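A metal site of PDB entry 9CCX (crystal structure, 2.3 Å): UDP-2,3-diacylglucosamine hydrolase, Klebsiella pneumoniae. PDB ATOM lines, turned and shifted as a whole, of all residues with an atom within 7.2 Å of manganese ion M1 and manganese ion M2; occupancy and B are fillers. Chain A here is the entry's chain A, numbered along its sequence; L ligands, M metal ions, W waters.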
ATOM      1  N   ALA A   7      36.264   5.344  13.902  1.00  0.00           N
ATOM      2  CA  ALA A   7      35.261   5.462  14.951  1.00  0.00           C
ATOM      3  C   ALA A   7      35.114   4.109  15.618  1.00  0.00           C
ATOM      4  O   ALA A   7      35.542   3.080  15.092  1.00  0.00           O
ATOM      5  CB  ALA A   7      33.904   5.930  14.408  1.00  0.00           C
ATOM      6  N   ASP A   8      34.515   4.144  16.813  1.00  0.00           N
ATOM      7  CA  ASP A   8      33.966   2.961  17.446  1.00  0.00           C
ATOM      8  C   ASP A   8      35.056   1.954  17.781  1.00  0.00           C
ATOM      9  O   ASP A   8      34.910   0.758  17.533  1.00  0.00           O
ATOM     10  CB  ASP A   8      32.894   2.320  16.563  1.00  0.00           C
ATOM     11  CG  ASP A   8      31.644   3.175  16.468  1.00  0.00           C
ATOM     12  OD1 ASP A   8      30.961   3.360  17.483  1.00  0.00           O
ATOM     13  OD2 ASP A   8      31.342   3.696  15.378  1.00  0.00           O
ATOM     14  N   LEU A   9      36.164   2.456  18.331  1.00  0.00           N
ATOM     15  CA  LEU A   9      37.266   1.618  18.786  1.00  0.00           C
ATOM     16  C   LEU A   9      36.957   0.989  20.141  1.00  0.00           C
ATOM     17  O   LEU A   9      37.383  -0.145  20.413  1.00  0.00           O
ATOM     18  CB  LEU A   9      38.526   2.456  18.881  1.00  0.00           C
ATOM     19  CG  LEU A   9      39.264   2.731  17.573  1.00  0.00           C
ATOM     20  CD1 LEU A   9      38.601   3.904  16.836  1.00  0.00           C
ATOM     21  CD2 LEU A   9      40.753   2.996  17.853  1.00  0.00           C
ATOM     22  N   HIS A  10      36.245   1.721  21.017  1.00  0.00           N
ATOM     23  CA  HIS A  10      35.885   1.231  22.345  1.00  0.00           C
ATOM     24  C   HIS A  10      37.107   0.774  23.149  1.00  0.00           C
ATOM     25  O   HIS A  10      37.111  -0.298  23.752  1.00  0.00           O
ATOM     26  CB  HIS A  10      34.858   0.098  22.245  1.00  0.00           C
ATOM     27  CG  HIS A  10      33.717   0.424  21.345  1.00  0.00           C
ATOM     28  ND1 HIS A  10      33.558  -0.147  20.103  1.00  0.00           N
ATOM     29  CD2 HIS A  10      32.675   1.274  21.501  1.00  0.00           C
ATOM     30  CE1 HIS A  10      32.468   0.328  19.536  1.00  0.00           C
ATOM     31  NE2 HIS A  10      31.912   1.205  20.360  1.00  0.00           N
ATOM     32  N   LEU A  39      35.284   9.902  14.908  1.00  0.00           N
ATOM     33  CA  LEU A  39      33.849  10.205  14.998  1.00  0.00           C
ATOM     34  C   LEU A  39      33.175   9.481  16.161  1.00  0.00           C
ATOM     35  O   LEU A  39      32.107   8.897  16.008  1.00  0.00           O
ATOM     36  CB  LEU A  39      33.170   9.860  13.673  1.00  0.00           C
ATOM     37  CG  LEU A  39      33.814  10.445  12.406  1.00  0.00           C
ATOM     38  CD1 LEU A  39      32.963  10.172  11.164  1.00  0.00           C
ATOM     39  CD2 LEU A  39      34.080  11.926  12.560  1.00  0.00           C
ATOM     40  N   GLY A  40      33.777   9.520  17.340  1.00  0.00           N
ATOM     41  CA  GLY A  40      33.099   9.083  18.543  1.00  0.00           C
ATOM     42  C   GLY A  40      33.373   7.626  18.886  1.00  0.00           C
ATOM     43  O   GLY A  40      33.749   6.809  18.040  1.00  0.00           O
ATOM     44  N   ASP A  41      33.146   7.306  20.171  1.00  0.00           N
ATOM     45  CA  ASP A  41      33.365   5.968  20.728  1.00  0.00           C
ATOM     46  C   ASP A  41      34.838   5.561  20.643  1.00  0.00           C
ATOM     47  O   ASP A  41      35.167   4.382  20.417  1.00  0.00           O
ATOM     48  CB  ASP A  41      32.479   4.897  20.066  1.00  0.00           C
ATOM     49  CG  ASP A  41      31.035   4.899  20.572  1.00  0.00           C
ATOM     50  OD1 ASP A  41      30.675   5.793  21.390  1.00  0.00           O
ATOM     51  OD2 ASP A  41      30.262   4.003  20.153  1.00  0.00           O
ATOM     52  N   GLU A  44      35.602   2.979  25.516  1.00  0.00           N
ATOM     53  CA  GLU A  44      34.414   2.232  25.917  1.00  0.00           C
ATOM     54  C   GLU A  44      33.607   2.958  26.993  1.00  0.00           C
ATOM     55  O   GLU A  44      32.393   2.731  27.116  1.00  0.00           O
ATOM     56  CB  GLU A  44      34.811   0.825  26.397  1.00  0.00           C
ATOM     57  CG  GLU A  44      33.691   0.024  27.060  1.00  0.00           C
ATOM     58  CD  GLU A  44      32.728  -0.581  26.050  1.00  0.00           C
ATOM     59  OE1 GLU A  44      32.793  -0.194  24.857  1.00  0.00           O
ATOM     60  OE2 GLU A  44      31.878  -1.410  26.452  1.00  0.00           O
ATOM     61  N   GLY A  78      31.041  10.333  20.882  1.00  0.00           N
ATOM     62  CA  GLY A  78      30.166   9.203  20.677  1.00  0.00           C
ATOM     63  C   GLY A  78      29.177   9.083  21.814  1.00  0.00           C
ATOM     64  O   GLY A  78      29.129   9.895  22.734  1.00  0.00           O
ATOM     65  N   ASN A  79      28.345   8.036  21.731  1.00  0.00           N
ATOM     66  CA  ASN A  79      27.411   7.820  22.823  1.00  0.00           C
ATOM     67  C   ASN A  79      28.098   7.251  24.059  1.00  0.00           C
ATOM     68  O   ASN A  79      27.586   7.431  25.166  1.00  0.00           O
ATOM     69  CB  ASN A  79      26.252   6.908  22.384  1.00  0.00           C
ATOM     70  CG  ASN A  79      26.701   5.507  22.015  1.00  0.00           C
ATOM     71  OD1 ASN A  79      27.443   5.310  21.054  1.00  0.00           O
ATOM     72  ND2 ASN A  79      26.202   4.514  22.750  1.00  0.00           N
ATOM     73  N   ARG A  80      29.258   6.616  23.895  1.00  0.00           N
ATOM     74  CA  ARG A  80      29.976   6.077  25.055  1.00  0.00           C
ATOM     75  C   ARG A  80      30.872   7.101  25.733  1.00  0.00           C
ATOM     76  O   ARG A  80      30.986   7.100  26.959  1.00  0.00           O
ATOM     77  CB  ARG A  80      30.823   4.857  24.647  1.00  0.00           C
ATOM     78  CG  ARG A  80      30.065   3.759  23.936  1.00  0.00           C
ATOM     79  CD  ARG A  80      28.989   3.135  24.819  1.00  0.00           C
ATOM     80  NE  ARG A  80      29.567   2.553  26.020  1.00  0.00           N
ATOM     81  CZ  ARG A  80      28.910   1.760  26.858  1.00  0.00           C
ATOM     82  NH1 ARG A  80      27.648   1.417  26.641  1.00  0.00           N
ATOM     83  NH2 ARG A  80      29.532   1.312  27.941  1.00  0.00           N
ATOM     84  N   ASP A  81      31.529   7.983  24.965  1.00  0.00           N
ATOM     85  CA  ASP A  81      32.528   8.893  25.530  1.00  0.00           C
ATOM     86  C   ASP A  81      32.117  10.361  25.391  1.00  0.00           C
ATOM     87  O   ASP A  81      32.956  11.245  25.180  1.00  0.00           O
ATOM     88  CB  ASP A  81      33.908   8.637  24.897  1.00  0.00           C
ATOM     89  CG  ASP A  81      33.852   8.478  23.357  1.00  0.00           C
ATOM     90  OD1 ASP A  81      32.828   8.824  22.723  1.00  0.00           O
ATOM     91  OD2 ASP A  81      34.855   8.000  22.793  1.00  0.00           O
ATOM     92  N   HIS A 114      28.636  11.195  14.609  1.00  0.00           N
ATOM     93  CA  HIS A 114      28.794   9.858  15.178  1.00  0.00           C
ATOM     94  C   HIS A 114      27.755   8.892  14.622  1.00  0.00           C
ATOM     95  O   HIS A 114      28.059   7.721  14.373  1.00  0.00           O
ATOM     96  CB  HIS A 114      28.698   9.894  16.709  1.00  0.00           C
ATOM     97  CG  HIS A 114      28.879   8.545  17.339  1.00  0.00           C
ATOM     98  ND1 HIS A 114      30.026   7.800  17.187  1.00  0.00           N
ATOM     99  CD2 HIS A 114      28.034   7.786  18.087  1.00  0.00           C
ATOM    100  CE1 HIS A 114      29.901   6.657  17.837  1.00  0.00           C
ATOM    101  NE2 HIS A 114      28.693   6.612  18.379  1.00  0.00           N
ATOM    102  N   GLY A 115      26.524   9.365  14.420  1.00  0.00           N
ATOM    103  CA  GLY A 115      25.457   8.562  13.862  1.00  0.00           C
ATOM    104  C   GLY A 115      24.394   8.127  14.854  1.00  0.00           C
ATOM    105  O   GLY A 115      23.361   7.599  14.426  1.00  0.00           O
ATOM    106  N   ASP A 116      24.581   8.329  16.152  1.00  0.00           N
ATOM    107  CA  ASP A 116      23.570   7.824  17.072  1.00  0.00           C
ATOM    108  C   ASP A 116      22.277   8.629  16.972  1.00  0.00           C
ATOM    109  O   ASP A 116      21.190   8.084  17.221  1.00  0.00           O
ATOM    110  CB  ASP A 116      24.087   7.775  18.518  1.00  0.00           C
ATOM    111  CG  ASP A 116      24.449   9.140  19.063  1.00  0.00           C
ATOM    112  OD1 ASP A 116      25.150   9.910  18.359  1.00  0.00           O
ATOM    113  OD2 ASP A 116      24.029   9.447  20.205  1.00  0.00           O
ATOM    114  N   TYR A 125      16.640   4.516  23.647  1.00  0.00           N
ATOM    115  CA  TYR A 125      17.938   5.170  23.613  1.00  0.00           C
ATOM    116  C   TYR A 125      17.803   6.682  23.629  1.00  0.00           C
ATOM    117  O   TYR A 125      18.555   7.376  24.330  1.00  0.00           O
ATOM    118  CB  TYR A 125      18.755   4.734  22.396  1.00  0.00           C
ATOM    119  CG  TYR A 125      19.986   5.601  22.248  1.00  0.00           C
ATOM    120  CD1 TYR A 125      20.980   5.570  23.218  1.00  0.00           C
ATOM    121  CD2 TYR A 125      20.168   6.428  21.148  1.00  0.00           C
ATOM    122  CE1 TYR A 125      22.111   6.368  23.131  1.00  0.00           C
ATOM    123  CE2 TYR A 125      21.299   7.221  21.033  1.00  0.00           C
ATOM    124  CZ  TYR A 125      22.266   7.186  22.033  1.00  0.00           C
ATOM    125  OH  TYR A 125      23.387   7.970  21.948  1.00  0.00           O
ATOM    126  N   GLY A 194      29.593   6.589  12.180  1.00  0.00           N
ATOM    127  CA  GLY A 194      29.821   5.265  12.734  1.00  0.00           C
ATOM    128  C   GLY A 194      28.635   4.794  13.551  1.00  0.00           C
ATOM    129  O   GLY A 194      27.506   4.736  13.047  1.00  0.00           O
ATOM    130  N   HIS A 195      28.902   4.434  14.811  1.00  0.00           N
ATOM    131  CA  HIS A 195      27.912   4.049  15.810  1.00  0.00           C
ATOM    132  C   HIS A 195      27.190   2.735  15.542  1.00  0.00           C
ATOM    133  O   HIS A 195      27.045   1.930  16.459  1.00  0.00           O
ATOM    134  CB  HIS A 195      26.850   5.125  15.996  1.00  0.00           C
ATOM    135  CG  HIS A 195      25.771   4.708  16.948  1.00  0.00           C
ATOM    136  ND1 HIS A 195      26.012   4.495  18.288  1.00  0.00           N
ATOM    137  CD2 HIS A 195      24.464   4.427  16.741  1.00  0.00           C
ATOM    138  CE1 HIS A 195      24.886   4.120  18.872  1.00  0.00           C
ATOM    139  NE2 HIS A 195      23.939   4.071  17.961  1.00  0.00           N
ATOM    140  N   THR A 196      26.694   2.519  14.312  1.00  0.00           N
ATOM    141  CA  THR A 196      25.935   1.291  14.049  1.00  0.00           C
ATOM    142  C   THR A 196      26.801   0.053  13.904  1.00  0.00           C
ATOM    143  O   THR A 196      26.253  -1.055  13.969  1.00  0.00           O
ATOM    144  CB  THR A 196      25.070   1.434  12.802  1.00  0.00           C
ATOM    145  OG1 THR A 196      25.915   1.639  11.653  1.00  0.00           O
ATOM    146  CG2 THR A 196      24.064   2.581  12.968  1.00  0.00           C
ATOM    147  N   HIS A 197      28.114   0.203  13.698  1.00  0.00           N
ATOM    148  CA  HIS A 197      29.015  -0.943  13.572  1.00  0.00           C
ATOM    149  C   HIS A 197      28.702  -1.796  12.336  1.00  0.00           C
ATOM    150  O   HIS A 197      29.002  -2.993  12.299  1.00  0.00           O
ATOM    151  CB  HIS A 197      28.994  -1.843  14.826  1.00  0.00           C
ATOM    152  CG  HIS A 197      29.387  -1.147  16.101  1.00  0.00           C
ATOM    153  ND1 HIS A 197      29.479  -1.821  17.301  1.00  0.00           N
ATOM    154  CD2 HIS A 197      29.736   0.136  16.359  1.00  0.00           C
ATOM    155  CE1 HIS A 197      29.841  -0.973  18.252  1.00  0.00           C
ATOM    156  NE2 HIS A 197      30.007   0.216  17.703  1.00  0.00           N
ATOM    157  N   ALA A 218      33.436  -1.028  13.588  1.00  0.00           N
ATOM    158  CA  ALA A 218      33.976  -1.130  14.936  1.00  0.00           C
ATOM    159  C   ALA A 218      35.242  -1.979  14.921  1.00  0.00           C
ATOM    160  O   ALA A 218      35.402  -2.866  14.069  1.00  0.00           O
ATOM    161  CB  ALA A 218      32.959  -1.762  15.887  1.00  0.00           C
HETATM  162  C1  LIG L   1      28.227   4.794  29.708  1.00  0.00           C
HETATM  163  C2  LIG L   1      27.115   5.077  27.587  1.00  0.00           C
HETATM  164  C3  LIG L   1      26.195   3.573  29.271  1.00  0.00           C
HETATM  165  C4  LIG L   1      24.291   2.636  28.100  1.00  0.00           C
HETATM  166  C5  LIG L   1      24.426   4.143  26.024  1.00  0.00           C
HETATM  167  C6  LIG L   1      23.158   3.541  25.431  1.00  0.00           C
HETATM  168  C7  LIG L   1      24.954  10.708  34.546  1.00  0.00           C
HETATM  169  C8  LIG L   1      23.916  10.508  35.639  1.00  0.00           C
HETATM  170  C9  LIG L   1      26.080  12.089  32.954  1.00  0.00           C
HETATM  171  C10 LIG L   1      26.695   9.874  33.158  1.00  0.00           C
HETATM  172  C11 LIG L   1      27.618   7.548  33.483  1.00  0.00           C
HETATM  173  C12 LIG L   1      27.872   6.368  32.565  1.00  0.00           C
HETATM  174  C13 LIG L   1      28.941   7.845  30.961  1.00  0.00           C
HETATM  175  C14 LIG L   1      28.696   9.021  31.902  1.00  0.00           C
HETATM  176  C15 LIG L   1      28.164   5.401  28.442  1.00  0.00           C
HETATM  177  C16 LIG L   1      26.129   4.168  28.000  1.00  0.00           C
HETATM  178  C17 LIG L   1      27.247   3.891  30.142  1.00  0.00           C
HETATM  179  C18 LIG L   1      24.987   2.642  29.432  1.00  0.00           C
HETATM  180  C19 LIG L   1      25.756   9.658  34.148  1.00  0.00           C
HETATM  181  C20 LIG L   1      25.121  11.950  33.936  1.00  0.00           C
HETATM  182  F1  LIG L   1      22.772  10.065  35.076  1.00  0.00           F
HETATM  183  F2  LIG L   1      24.329   9.573  36.563  1.00  0.00           F
HETATM  184  F3  LIG L   1      23.701  11.707  36.252  1.00  0.00           F
HETATM  185  N1  LIG L   1      26.838  11.064  32.601  1.00  0.00           N
HETATM  186  N2  LIG L   1      27.525   8.784  32.725  1.00  0.00           N
HETATM  187  N3  LIG L   1      29.012   6.579  31.667  1.00  0.00           N
HETATM  188  N4  LIG L   1      24.911   3.661  27.305  1.00  0.00           N
HETATM  189  O1  LIG L   1      29.953   4.104  31.697  1.00  0.00           O
HETATM  190  O2  LIG L   1      30.826   5.539  30.082  1.00  0.00           O
HETATM  191  O3  LIG L   1      25.030   4.989  25.448  1.00  0.00           O
HETATM  192  S1  LIG L   1      29.594   5.229  30.810  1.00  0.00           S
HETATM  193 MN    MN M   1      30.298   2.103  19.005  1.00  0.00          MN
HETATM  194 MN    MN M   2      28.176   4.585  19.342  1.00  0.00          MN
HETATM  195  O   HOH W   1      28.148   2.455  18.969  1.00  0.00           O
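ND2 of Asn 79 is in hydrogen-bond range of O3 of the ligand, 3.0 Å away.
The side-chain carboxylate (OD2) of Asp 8 is in hydrogen-bond range of the backbone NH (N) of His 195 (2.6 Å). The backbone carbonyl oxygen (O) of Gly 40 lies within hydrogen-bond range of the backbone NH (N) of Asp 8. The backbone NH (N) of Arg 80 is in hydrogen-bond range of the side-chain carboxylate (OD1) of Asp 41, 3.0 Å away. The backbone carbonyl oxygen of Asp 41 lies within hydrogen-bond range of the backbone NH of Leu 9. OD1 of Asp 81 is in hydrogen-bond range of N of Asp 41 (3.0 Å). O of His 114 lies within hydrogen-bond range of N of Gly 194, 2.9 Å away. A ring nitrogen (ND1) of His 114 is in hydrogen-bond range of the backbone carbonyl oxygen (O) of Leu 39.
Four residues have an atom within 4 Å of manganese ion M1: Asp 8, His 10, Asp 41 and His 197. The nearest printed residue that does not touch manganese ion M1 is His 195 (4.1 Å).
Within 4 Å of manganese ion M2: Asp 8, Asp 41, Asn 79, His 114 and His 195.
Manganese ion M1 is bound by the side-chain carboxylate of Asp 8 (2.1 Å), water W1 (2.2 Å), the side-chain carboxylate of Asp 41 (2.2 Å), a ring nitrogen (NE2) of His 10 (2.3 Å) and a ring nitrogen (NE2) of His 197 (2.3 Å). Manganese ion M1 has five donor atoms within binding distance.
Manganese ion M2 is bound by the side-chain amide oxygen (OD1) of Asn 79, at 2.0 Å. Manganese ion M2 is bound by water W1, at 2.2 Å. A ring nitrogen (NE2) of His 114 is bound to manganese ion M2 (2.3 Å). Manganese ion M2 is bound by OD2 of Asp 41, at 2.3 Å. Manganese ion M2 is bound by ND1 of His 195 (2.4 Å).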
